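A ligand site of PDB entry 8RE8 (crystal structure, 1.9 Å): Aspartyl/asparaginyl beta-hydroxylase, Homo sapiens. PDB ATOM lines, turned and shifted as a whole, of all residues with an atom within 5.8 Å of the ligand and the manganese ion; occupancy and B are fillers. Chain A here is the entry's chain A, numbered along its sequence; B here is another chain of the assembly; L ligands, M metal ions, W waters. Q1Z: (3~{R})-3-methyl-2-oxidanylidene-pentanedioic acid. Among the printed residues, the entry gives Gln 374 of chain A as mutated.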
ATOM      1  N   LEU A 305      10.233  27.303   7.540  1.00  0.00           N
ATOM      2  CA  LEU A 305      11.364  27.295   8.461  1.00  0.00           C
ATOM      3  C   LEU A 305      11.720  25.893   8.956  1.00  0.00           C
ATOM      4  O   LEU A 305      12.723  25.744   9.675  1.00  0.00           O
ATOM      5  CB  LEU A 305      11.074  28.195   9.663  1.00  0.00           C
ATOM      6  CG  LEU A 305      10.964  29.696   9.359  1.00  0.00           C
ATOM      7  CD1 LEU A 305      10.650  30.463  10.618  1.00  0.00           C
ATOM      8  CD2 LEU A 305      12.251  30.212   8.735  1.00  0.00           C
ATOM      9  N   TRP A 311       5.298  21.553  13.852  1.00  0.00           N
ATOM     10  CA  TRP A 311       5.460  22.736  14.678  1.00  0.00           C
ATOM     11  C   TRP A 311       4.268  23.632  14.381  1.00  0.00           C
ATOM     12  O   TRP A 311       4.046  23.995  13.214  1.00  0.00           O
ATOM     13  CB  TRP A 311       6.786  23.438  14.365  1.00  0.00           C
ATOM     14  CG  TRP A 311       6.992  24.807  14.963  1.00  0.00           C
ATOM     15  CD1 TRP A 311       6.416  25.324  16.087  1.00  0.00           C
ATOM     16  CD2 TRP A 311       7.853  25.838  14.443  1.00  0.00           C
ATOM     17  NE1 TRP A 311       6.873  26.608  16.306  1.00  0.00           N
ATOM     18  CE2 TRP A 311       7.755  26.939  15.308  1.00  0.00           C
ATOM     19  CE3 TRP A 311       8.698  25.914  13.332  1.00  0.00           C
ATOM     20  CZ2 TRP A 311       8.461  28.130  15.091  1.00  0.00           C
ATOM     21  CZ3 TRP A 311       9.410  27.096  13.121  1.00  0.00           C
ATOM     22  CH2 TRP A 311       9.285  28.180  14.001  1.00  0.00           C
ATOM     23  N   GLN A 313       1.468  26.862  16.143  1.00  0.00           N
ATOM     24  CA  GLN A 313       1.418  27.981  17.068  1.00  0.00           C
ATOM     25  C   GLN A 313      -0.007  28.480  17.229  1.00  0.00           C
ATOM     26  O   GLN A 313      -0.798  28.490  16.279  1.00  0.00           O
ATOM     27  CB  GLN A 313       2.360  29.111  16.594  1.00  0.00           C
ATOM     28  CG  GLN A 313       3.835  28.655  16.576  1.00  0.00           C
ATOM     29  CD  GLN A 313       4.829  29.742  16.224  1.00  0.00           C
ATOM     30  OE1 GLN A 313       5.719  30.056  17.024  1.00  0.00           O
ATOM     31  NE2 GLN A 313       4.714  30.295  15.027  1.00  0.00           N
ATOM     32  N   SER A 354       3.528  27.643  21.446  1.00  0.00           N
ATOM     33  CA  SER A 354       4.286  27.011  20.369  1.00  0.00           C
ATOM     34  C   SER A 354       4.503  25.550  20.725  1.00  0.00           C
ATOM     35  O   SER A 354       5.236  25.238  21.675  1.00  0.00           O
ATOM     36  CB  SER A 354       5.629  27.718  20.153  1.00  0.00           C
ATOM     37  OG  SER A 354       6.313  27.206  19.021  1.00  0.00           O
ATOM     38  N   ILE A 355       3.890  24.643  19.965  1.00  0.00           N
ATOM     39  CA  ILE A 355       4.052  23.218  20.205  1.00  0.00           C
ATOM     40  C   ILE A 355       4.943  22.643  19.114  1.00  0.00           C
ATOM     41  O   ILE A 355       4.828  23.004  17.930  1.00  0.00           O
ATOM     42  CB  ILE A 355       2.685  22.490  20.285  1.00  0.00           C
ATOM     43  CG1 ILE A 355       2.858  21.097  20.883  1.00  0.00           C
ATOM     44  CG2 ILE A 355       2.029  22.395  18.926  1.00  0.00           C
ATOM     45  CD1 ILE A 355       1.545  20.358  21.059  1.00  0.00           C
ATOM     46  N   MET A 356       5.857  21.756  19.518  1.00  0.00           N
ATOM     47  CA  MET A 356       6.761  21.098  18.596  1.00  0.00           C
ATOM     48  C   MET A 356       6.849  19.631  18.963  1.00  0.00           C
ATOM     49  O   MET A 356       6.936  19.283  20.150  1.00  0.00           O
ATOM     50  CB  MET A 356       8.148  21.740  18.636  1.00  0.00           C
ATOM     51  CG  MET A 356       9.058  21.296  17.516  1.00  0.00           C
ATOM     52  SD  MET A 356      10.603  22.205  17.528  1.00  0.00           S
ATOM     53  CE  MET A 356      10.017  23.869  17.191  1.00  0.00           C
ATOM     54  N   VAL A 362      14.142  22.843  13.036  1.00  0.00           N
ATOM     55  CA  VAL A 362      13.912  24.182  12.509  1.00  0.00           C
ATOM     56  C   VAL A 362      15.232  24.692  11.926  1.00  0.00           C
ATOM     57  O   VAL A 362      16.245  24.726  12.626  1.00  0.00           O
ATOM     58  CB  VAL A 362      13.383  25.133  13.591  1.00  0.00           C
ATOM     59  CG1 VAL A 362      13.109  26.524  13.023  1.00  0.00           C
ATOM     60  CG2 VAL A 362      12.131  24.538  14.251  1.00  0.00           C
ATOM     61  N   HIS A 365      17.762  30.339  11.360  1.00  0.00           N
ATOM     62  CA  HIS A 365      17.094  31.491  10.772  1.00  0.00           C
ATOM     63  C   HIS A 365      17.203  32.671  11.718  1.00  0.00           C
ATOM     64  O   HIS A 365      17.604  32.545  12.881  1.00  0.00           O
ATOM     65  CB  HIS A 365      15.625  31.203  10.463  1.00  0.00           C
ATOM     66  CG  HIS A 365      14.780  30.996  11.680  1.00  0.00           C
ATOM     67  ND1 HIS A 365      14.811  29.819  12.406  1.00  0.00           N
ATOM     68  CD2 HIS A 365      13.906  31.817  12.303  1.00  0.00           C
ATOM     69  CE1 HIS A 365      13.975  29.927  13.434  1.00  0.00           C
ATOM     70  NE2 HIS A 365      13.418  31.130  13.390  1.00  0.00           N
ATOM     71  N   GLY A 367      15.008  36.443  12.850  1.00  0.00           N
ATOM     72  CA  GLY A 367      13.787  37.221  12.791  1.00  0.00           C
ATOM     73  C   GLY A 367      13.982  38.498  12.000  1.00  0.00           C
ATOM     74  O   GLY A 367      15.090  38.899  11.643  1.00  0.00           O
ATOM     75  N   GLN A 374      12.732  38.066  22.839  1.00  0.00           N
ATOM     76  CA  GLN A 374      11.798  36.967  22.876  1.00  0.00           C
ATOM     77  C   GLN A 374      11.960  36.171  24.164  1.00  0.00           C
ATOM     78  O   GLN A 374      13.045  35.661  24.450  1.00  0.00           O
ATOM     79  CB  GLN A 374      11.990  36.047  21.669  1.00  0.00           C
ATOM     80  CG  GLN A 374      10.889  35.040  21.538  1.00  0.00           C
ATOM     81  CD  GLN A 374      10.764  34.538  20.124  1.00  0.00           C
ATOM     82  OE1 GLN A 374      11.275  33.481  19.795  1.00  0.00           O
ATOM     83  NE2 GLN A 374      10.090  35.299  19.271  1.00  0.00           N
ATOM     84  N   HIS A 376      10.778  32.823  26.289  1.00  0.00           N
ATOM     85  CA  HIS A 376      10.201  31.480  26.187  1.00  0.00           C
ATOM     86  C   HIS A 376       9.933  31.000  27.599  1.00  0.00           C
ATOM     87  O   HIS A 376      10.860  30.901  28.409  1.00  0.00           O
ATOM     88  CB  HIS A 376      11.151  30.504  25.494  1.00  0.00           C
ATOM     89  CG  HIS A 376      11.219  30.647  24.002  1.00  0.00           C
ATOM     90  ND1 HIS A 376      11.889  29.742  23.211  1.00  0.00           N
ATOM     91  CD2 HIS A 376      10.702  31.574  23.164  1.00  0.00           C
ATOM     92  CE1 HIS A 376      11.787  30.103  21.950  1.00  0.00           C
ATOM     93  NE2 HIS A 376      11.074  31.220  21.891  1.00  0.00           N
ATOM     94  N   ILE A 388      17.620  24.531  21.915  1.00  0.00           N
ATOM     95  CA  ILE A 388      17.623  25.708  21.058  1.00  0.00           C
ATOM     96  C   ILE A 388      19.021  26.300  21.074  1.00  0.00           C
ATOM     97  O   ILE A 388      19.615  26.491  22.141  1.00  0.00           O
ATOM     98  CB  ILE A 388      16.572  26.747  21.514  1.00  0.00           C
ATOM     99  CG1 ILE A 388      16.740  28.056  20.750  1.00  0.00           C
ATOM    100  CG2 ILE A 388      16.624  26.953  23.028  1.00  0.00           C
ATOM    101  CD1 ILE A 388      15.554  29.013  20.892  1.00  0.00           C
ATOM    102  N   TRP A 397      14.980  24.312  27.571  1.00  0.00           N
ATOM    103  CA  TRP A 397      13.926  24.913  28.366  1.00  0.00           C
ATOM    104  C   TRP A 397      13.747  24.146  29.670  1.00  0.00           C
ATOM    105  O   TRP A 397      14.133  22.988  29.801  1.00  0.00           O
ATOM    106  CB  TRP A 397      12.613  24.924  27.592  1.00  0.00           C
ATOM    107  CG  TRP A 397      12.666  25.654  26.297  1.00  0.00           C
ATOM    108  CD1 TRP A 397      12.368  26.971  26.073  1.00  0.00           C
ATOM    109  CD2 TRP A 397      13.001  25.107  25.002  1.00  0.00           C
ATOM    110  NE1 TRP A 397      12.506  27.282  24.738  1.00  0.00           N
ATOM    111  CE2 TRP A 397      12.889  26.154  24.062  1.00  0.00           C
ATOM    112  CE3 TRP A 397      13.381  23.833  24.559  1.00  0.00           C
ATOM    113  CZ2 TRP A 397      13.154  25.976  22.704  1.00  0.00           C
ATOM    114  CZ3 TRP A 397      13.645  23.655  23.201  1.00  0.00           C
ATOM    115  CH2 TRP A 397      13.531  24.714  22.291  1.00  0.00           C
ATOM    116  N   PHE A 405      16.085  35.481  24.656  1.00  0.00           N
ATOM    117  CA  PHE A 405      17.109  35.662  23.644  1.00  0.00           C
ATOM    118  C   PHE A 405      16.626  36.678  22.618  1.00  0.00           C
ATOM    119  O   PHE A 405      15.437  37.005  22.535  1.00  0.00           O
ATOM    120  CB  PHE A 405      17.494  34.337  22.960  1.00  0.00           C
ATOM    121  CG  PHE A 405      16.412  33.739  22.101  1.00  0.00           C
ATOM    122  CD1 PHE A 405      15.343  33.060  22.667  1.00  0.00           C
ATOM    123  CD2 PHE A 405      16.487  33.816  20.714  1.00  0.00           C
ATOM    124  CE1 PHE A 405      14.354  32.497  21.878  1.00  0.00           C
ATOM    125  CE2 PHE A 405      15.510  33.258  19.921  1.00  0.00           C
ATOM    126  CZ  PHE A 405      14.442  32.592  20.502  1.00  0.00           C
ATOM    127  N   ASP A 407      16.033  37.078  18.972  1.00  0.00           N
ATOM    128  CA  ASP A 407      15.881  36.229  17.799  1.00  0.00           C
ATOM    129  C   ASP A 407      16.285  36.934  16.495  1.00  0.00           C
ATOM    130  O   ASP A 407      16.138  36.335  15.430  1.00  0.00           O
ATOM    131  CB  ASP A 407      14.451  35.676  17.715  1.00  0.00           C
ATOM    132  CG  ASP A 407      13.460  36.616  17.040  1.00  0.00           C
ATOM    133  OD1 ASP A 407      13.579  37.850  17.199  1.00  0.00           O
ATOM    134  OD2 ASP A 407      12.548  36.107  16.372  1.00  0.00           O
ATOM    135  N   HIS A 411      19.227  31.529  15.040  1.00  0.00           N
ATOM    136  CA  HIS A 411      18.869  30.509  16.016  1.00  0.00           C
ATOM    137  C   HIS A 411      18.275  29.306  15.301  1.00  0.00           C
ATOM    138  O   HIS A 411      17.859  29.377  14.145  1.00  0.00           O
ATOM    139  CB  HIS A 411      17.920  31.056  17.094  1.00  0.00           C
ATOM    140  CG  HIS A 411      16.680  31.688  16.549  1.00  0.00           C
ATOM    141  ND1 HIS A 411      16.679  32.918  15.920  1.00  0.00           N
ATOM    142  CD2 HIS A 411      15.387  31.267  16.545  1.00  0.00           C
ATOM    143  CE1 HIS A 411      15.447  33.212  15.545  1.00  0.00           C
ATOM    144  NE2 HIS A 411      14.644  32.229  15.920  1.00  0.00           N
ATOM    145  N   VAL A 413      16.478  25.117  16.217  1.00  0.00           N
ATOM    146  CA  VAL A 413      15.806  24.316  17.224  1.00  0.00           C
ATOM    147  C   VAL A 413      15.705  22.869  16.748  1.00  0.00           C
ATOM    148  O   VAL A 413      15.467  22.600  15.562  1.00  0.00           O
ATOM    149  CB  VAL A 413      14.403  24.885  17.546  1.00  0.00           C
ATOM    150  CG1 VAL A 413      13.626  23.945  18.463  1.00  0.00           C
ATOM    151  CG2 VAL A 413      14.533  26.242  18.208  1.00  0.00           C
ATOM    152  N   ARG A 421       6.480  18.923  23.052  1.00  0.00           N
ATOM    153  CA  ARG A 421       7.116  19.994  23.807  1.00  0.00           C
ATOM    154  C   ARG A 421       6.315  21.270  23.586  1.00  0.00           C
ATOM    155  O   ARG A 421       6.180  21.747  22.451  1.00  0.00           O
ATOM    156  CB  ARG A 421       8.565  20.205  23.369  1.00  0.00           C
ATOM    157  CG  ARG A 421       9.276  21.348  24.101  1.00  0.00           C
ATOM    158  CD  ARG A 421       9.864  22.364  23.118  1.00  0.00           C
ATOM    159  NE  ARG A 421       8.822  23.074  22.387  1.00  0.00           N
ATOM    160  CZ  ARG A 421       9.045  24.053  21.527  1.00  0.00           C
ATOM    161  NH1 ARG A 421      10.269  24.455  21.227  1.00  0.00           N
ATOM    162  NH2 ARG A 421       8.014  24.649  20.925  1.00  0.00           N
ATOM    163  N   ILE A 423       5.790  25.331  24.697  1.00  0.00           N
ATOM    164  CA  ILE A 423       6.324  26.529  25.328  1.00  0.00           C
ATOM    165  C   ILE A 423       5.372  27.692  25.076  1.00  0.00           C
ATOM    166  O   ILE A 423       4.493  27.630  24.226  1.00  0.00           O
ATOM    167  CB  ILE A 423       7.756  26.896  24.856  1.00  0.00           C
ATOM    168  CG1 ILE A 423       7.743  27.255  23.374  1.00  0.00           C
ATOM    169  CG2 ILE A 423       8.738  25.763  25.159  1.00  0.00           C
ATOM    170  CD1 ILE A 423       9.068  27.853  22.900  1.00  0.00           C
ATOM    171  N   ILE A 425       5.531  31.773  24.202  1.00  0.00           N
ATOM    172  CA  ILE A 425       6.459  32.743  23.626  1.00  0.00           C
ATOM    173  C   ILE A 425       5.900  34.141  23.836  1.00  0.00           C
ATOM    174  O   ILE A 425       4.765  34.429  23.435  1.00  0.00           O
ATOM    175  CB  ILE A 425       6.708  32.462  22.134  1.00  0.00           C
ATOM    176  CG1 ILE A 425       7.281  31.056  21.955  1.00  0.00           C
ATOM    177  CG2 ILE A 425       7.658  33.515  21.555  1.00  0.00           C
ATOM    178  CD1 ILE A 425       7.627  30.694  20.512  1.00  0.00           C
ATOM    179  N   ASP B  18       8.264  34.769  12.408  1.00  0.00           N
ATOM    180  CA  ASP B  18       9.550  34.224  12.816  1.00  0.00           C
ATOM    181  C   ASP B  18      10.671  34.517  11.839  1.00  0.00           C
ATOM    182  O   ASP B  18      11.833  34.537  12.248  1.00  0.00           O
ATOM    183  CB  ASP B  18       9.459  32.707  12.986  1.00  0.00           C
ATOM    184  CG  ASP B  18       9.022  32.316  14.359  1.00  0.00           C
ATOM    185  OD1 ASP B  18       7.794  32.303  14.602  1.00  0.00           O
ATOM    186  OD2 ASP B  18       9.905  32.033  15.203  1.00  0.00           O
HETATM  187  C01 Q1Z L   1      11.707  29.868  17.123  1.00  0.00           C
HETATM  188  C02 Q1Z L   1      11.400  28.487  17.732  1.00  0.00           C
HETATM  189  C03 Q1Z L   1       9.954  28.406  18.232  1.00  0.00           C
HETATM  190  C04 Q1Z L   1      11.605  27.448  16.633  1.00  0.00           C
HETATM  191  C05 Q1Z L   1      11.584  31.133  17.960  1.00  0.00           C
HETATM  192  C06 Q1Z L   1       9.797  27.211  19.174  1.00  0.00           C
HETATM  193  O01 Q1Z L   1      12.052  29.942  15.995  1.00  0.00           O
HETATM  194  O02 Q1Z L   1      11.899  32.268  17.483  1.00  0.00           O
HETATM  195  O03 Q1Z L   1      11.156  31.013  19.140  1.00  0.00           O
HETATM  196  O04 Q1Z L   1       8.646  26.818  19.488  1.00  0.00           O
HETATM  197  O05 Q1Z L   1      10.810  26.621  19.643  1.00  0.00           O
HETATM  198 MN    MN M   1      12.560  31.983  15.347  1.00  0.00          MN
HETATM  199  O   HOH W   1      12.548  34.058  14.668  1.00  0.00           O
HETATM  200  O   HOH W   2       8.580  31.380  17.275  1.00  0.00           O
HETATM  201  O   HOH W   3       9.507  34.338  16.629  1.00  0.00           O
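The side-chain hydroxyl of Ser 354 sits at hydrogen-bond distance from an oxygen (O04) of the ligand, at 2.4 Å.
NE2 of His 376 lies within hydrogen-bond range of O03 of the ligand (2.8 Å).
NH2 of Arg 421 lies within salt-bridge range of O04 of the ligand.
O03 of the ligand sits close to OE1 of Gln 374, 2.6 Å away.
The backbone NH (N) of Ser 354 is in hydrogen-bond range of the backbone carbonyl oxygen (O) of Ile 423 (2.9 Å).
OE1 of Gln 374 sits at hydrogen-bond distance from NE2 of His 376, at 3.1 Å.
The backbone carbonyl oxygen of Val 413 is in hydrogen-bond range of the backbone NH of Val 362, 2.9 Å away.
The indole nitrogen of Trp 311 lies within hydrogen-bond range of the side-chain hydroxyl of Ser 354.
The backbone carbonyl oxygen (O) of Arg 421 is in hydrogen-bond range of the backbone NH (N) of Met 356, at 3.0 Å.
ND1 of His 376 is in hydrogen-bond range of NE1 of Trp 397 (3.0 Å).
The backbone carbonyl oxygen (O) of Phe 405 is in hydrogen-bond range of the backbone NH (N) of Gln 374.
O of Asp 407 lies close to ND1 of His 411 (3.5 Å).
CZ2 of Trp 311 touches C03 of the ligand, 3.5 Å away.
Met 356 touches the ligand (CE to O05, 3.8 Å).
Val 362 touches the ligand (CG2 to C04, 3.8 Å).
Trp 397 touches the ligand (CZ2 to O05, 3.9 Å).
Phe 405 touches the ligand.
Val 413 touches the ligand.
CD1 of Ile 423 touches O04 of the ligand (3.6 Å).
CD1 of Ile 425 touches O03 of the ligand, 3.8 Å away.
Hydrophobic or aromatic side chains that line the ligand: Trp 311, Met 356, Val 362, His 365, His 376, Trp 397, Phe 405, His 411, Val 413, Ile 423 and Ile 425.
15 residues have an atom within 4 Å of the ligand: Trp 311, Ser 354, Met 356, Val 362, His 365, Gln 374, His 376, Trp 397, Phe 405, His 411, Val 413, Arg 421, Ile 423, Ile 425 and Asp 18 of chain B.
The nearest printed residue that does not touch the ligand is Asp 407 (4.05 Å).
Of the 21 residues printed, 3 come within 4 Å of the manganese ion.
The manganese ion is bound by NE2 of His 411 (2.2 Å), water W1 (2.2 Å), O01 of the ligand (2.2 Å), O02 of the ligand (2.3 Å), NE2 of His 365 (2.3 Å) and OD2 of Asp 18 of chain B (2.7 Å).
The manganese ion has six donor atoms within binding distance.
Water W1 lies within hydrogen-bond range of O of Asp 18 of chain B (2.6 Å) and OD2 of Asp 407 (2.7 Å).
Water W2 lies within hydrogen-bond range of the side-chain carboxylate of Asp 18 of chain B, the side-chain amide oxygen of Gln 313 and an oxygen (O03) of the ligand.
Water W3 bridges the side-chain amide nitrogen of Gln 374 and the side-chain carboxylate of Asp 18 of chain B.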
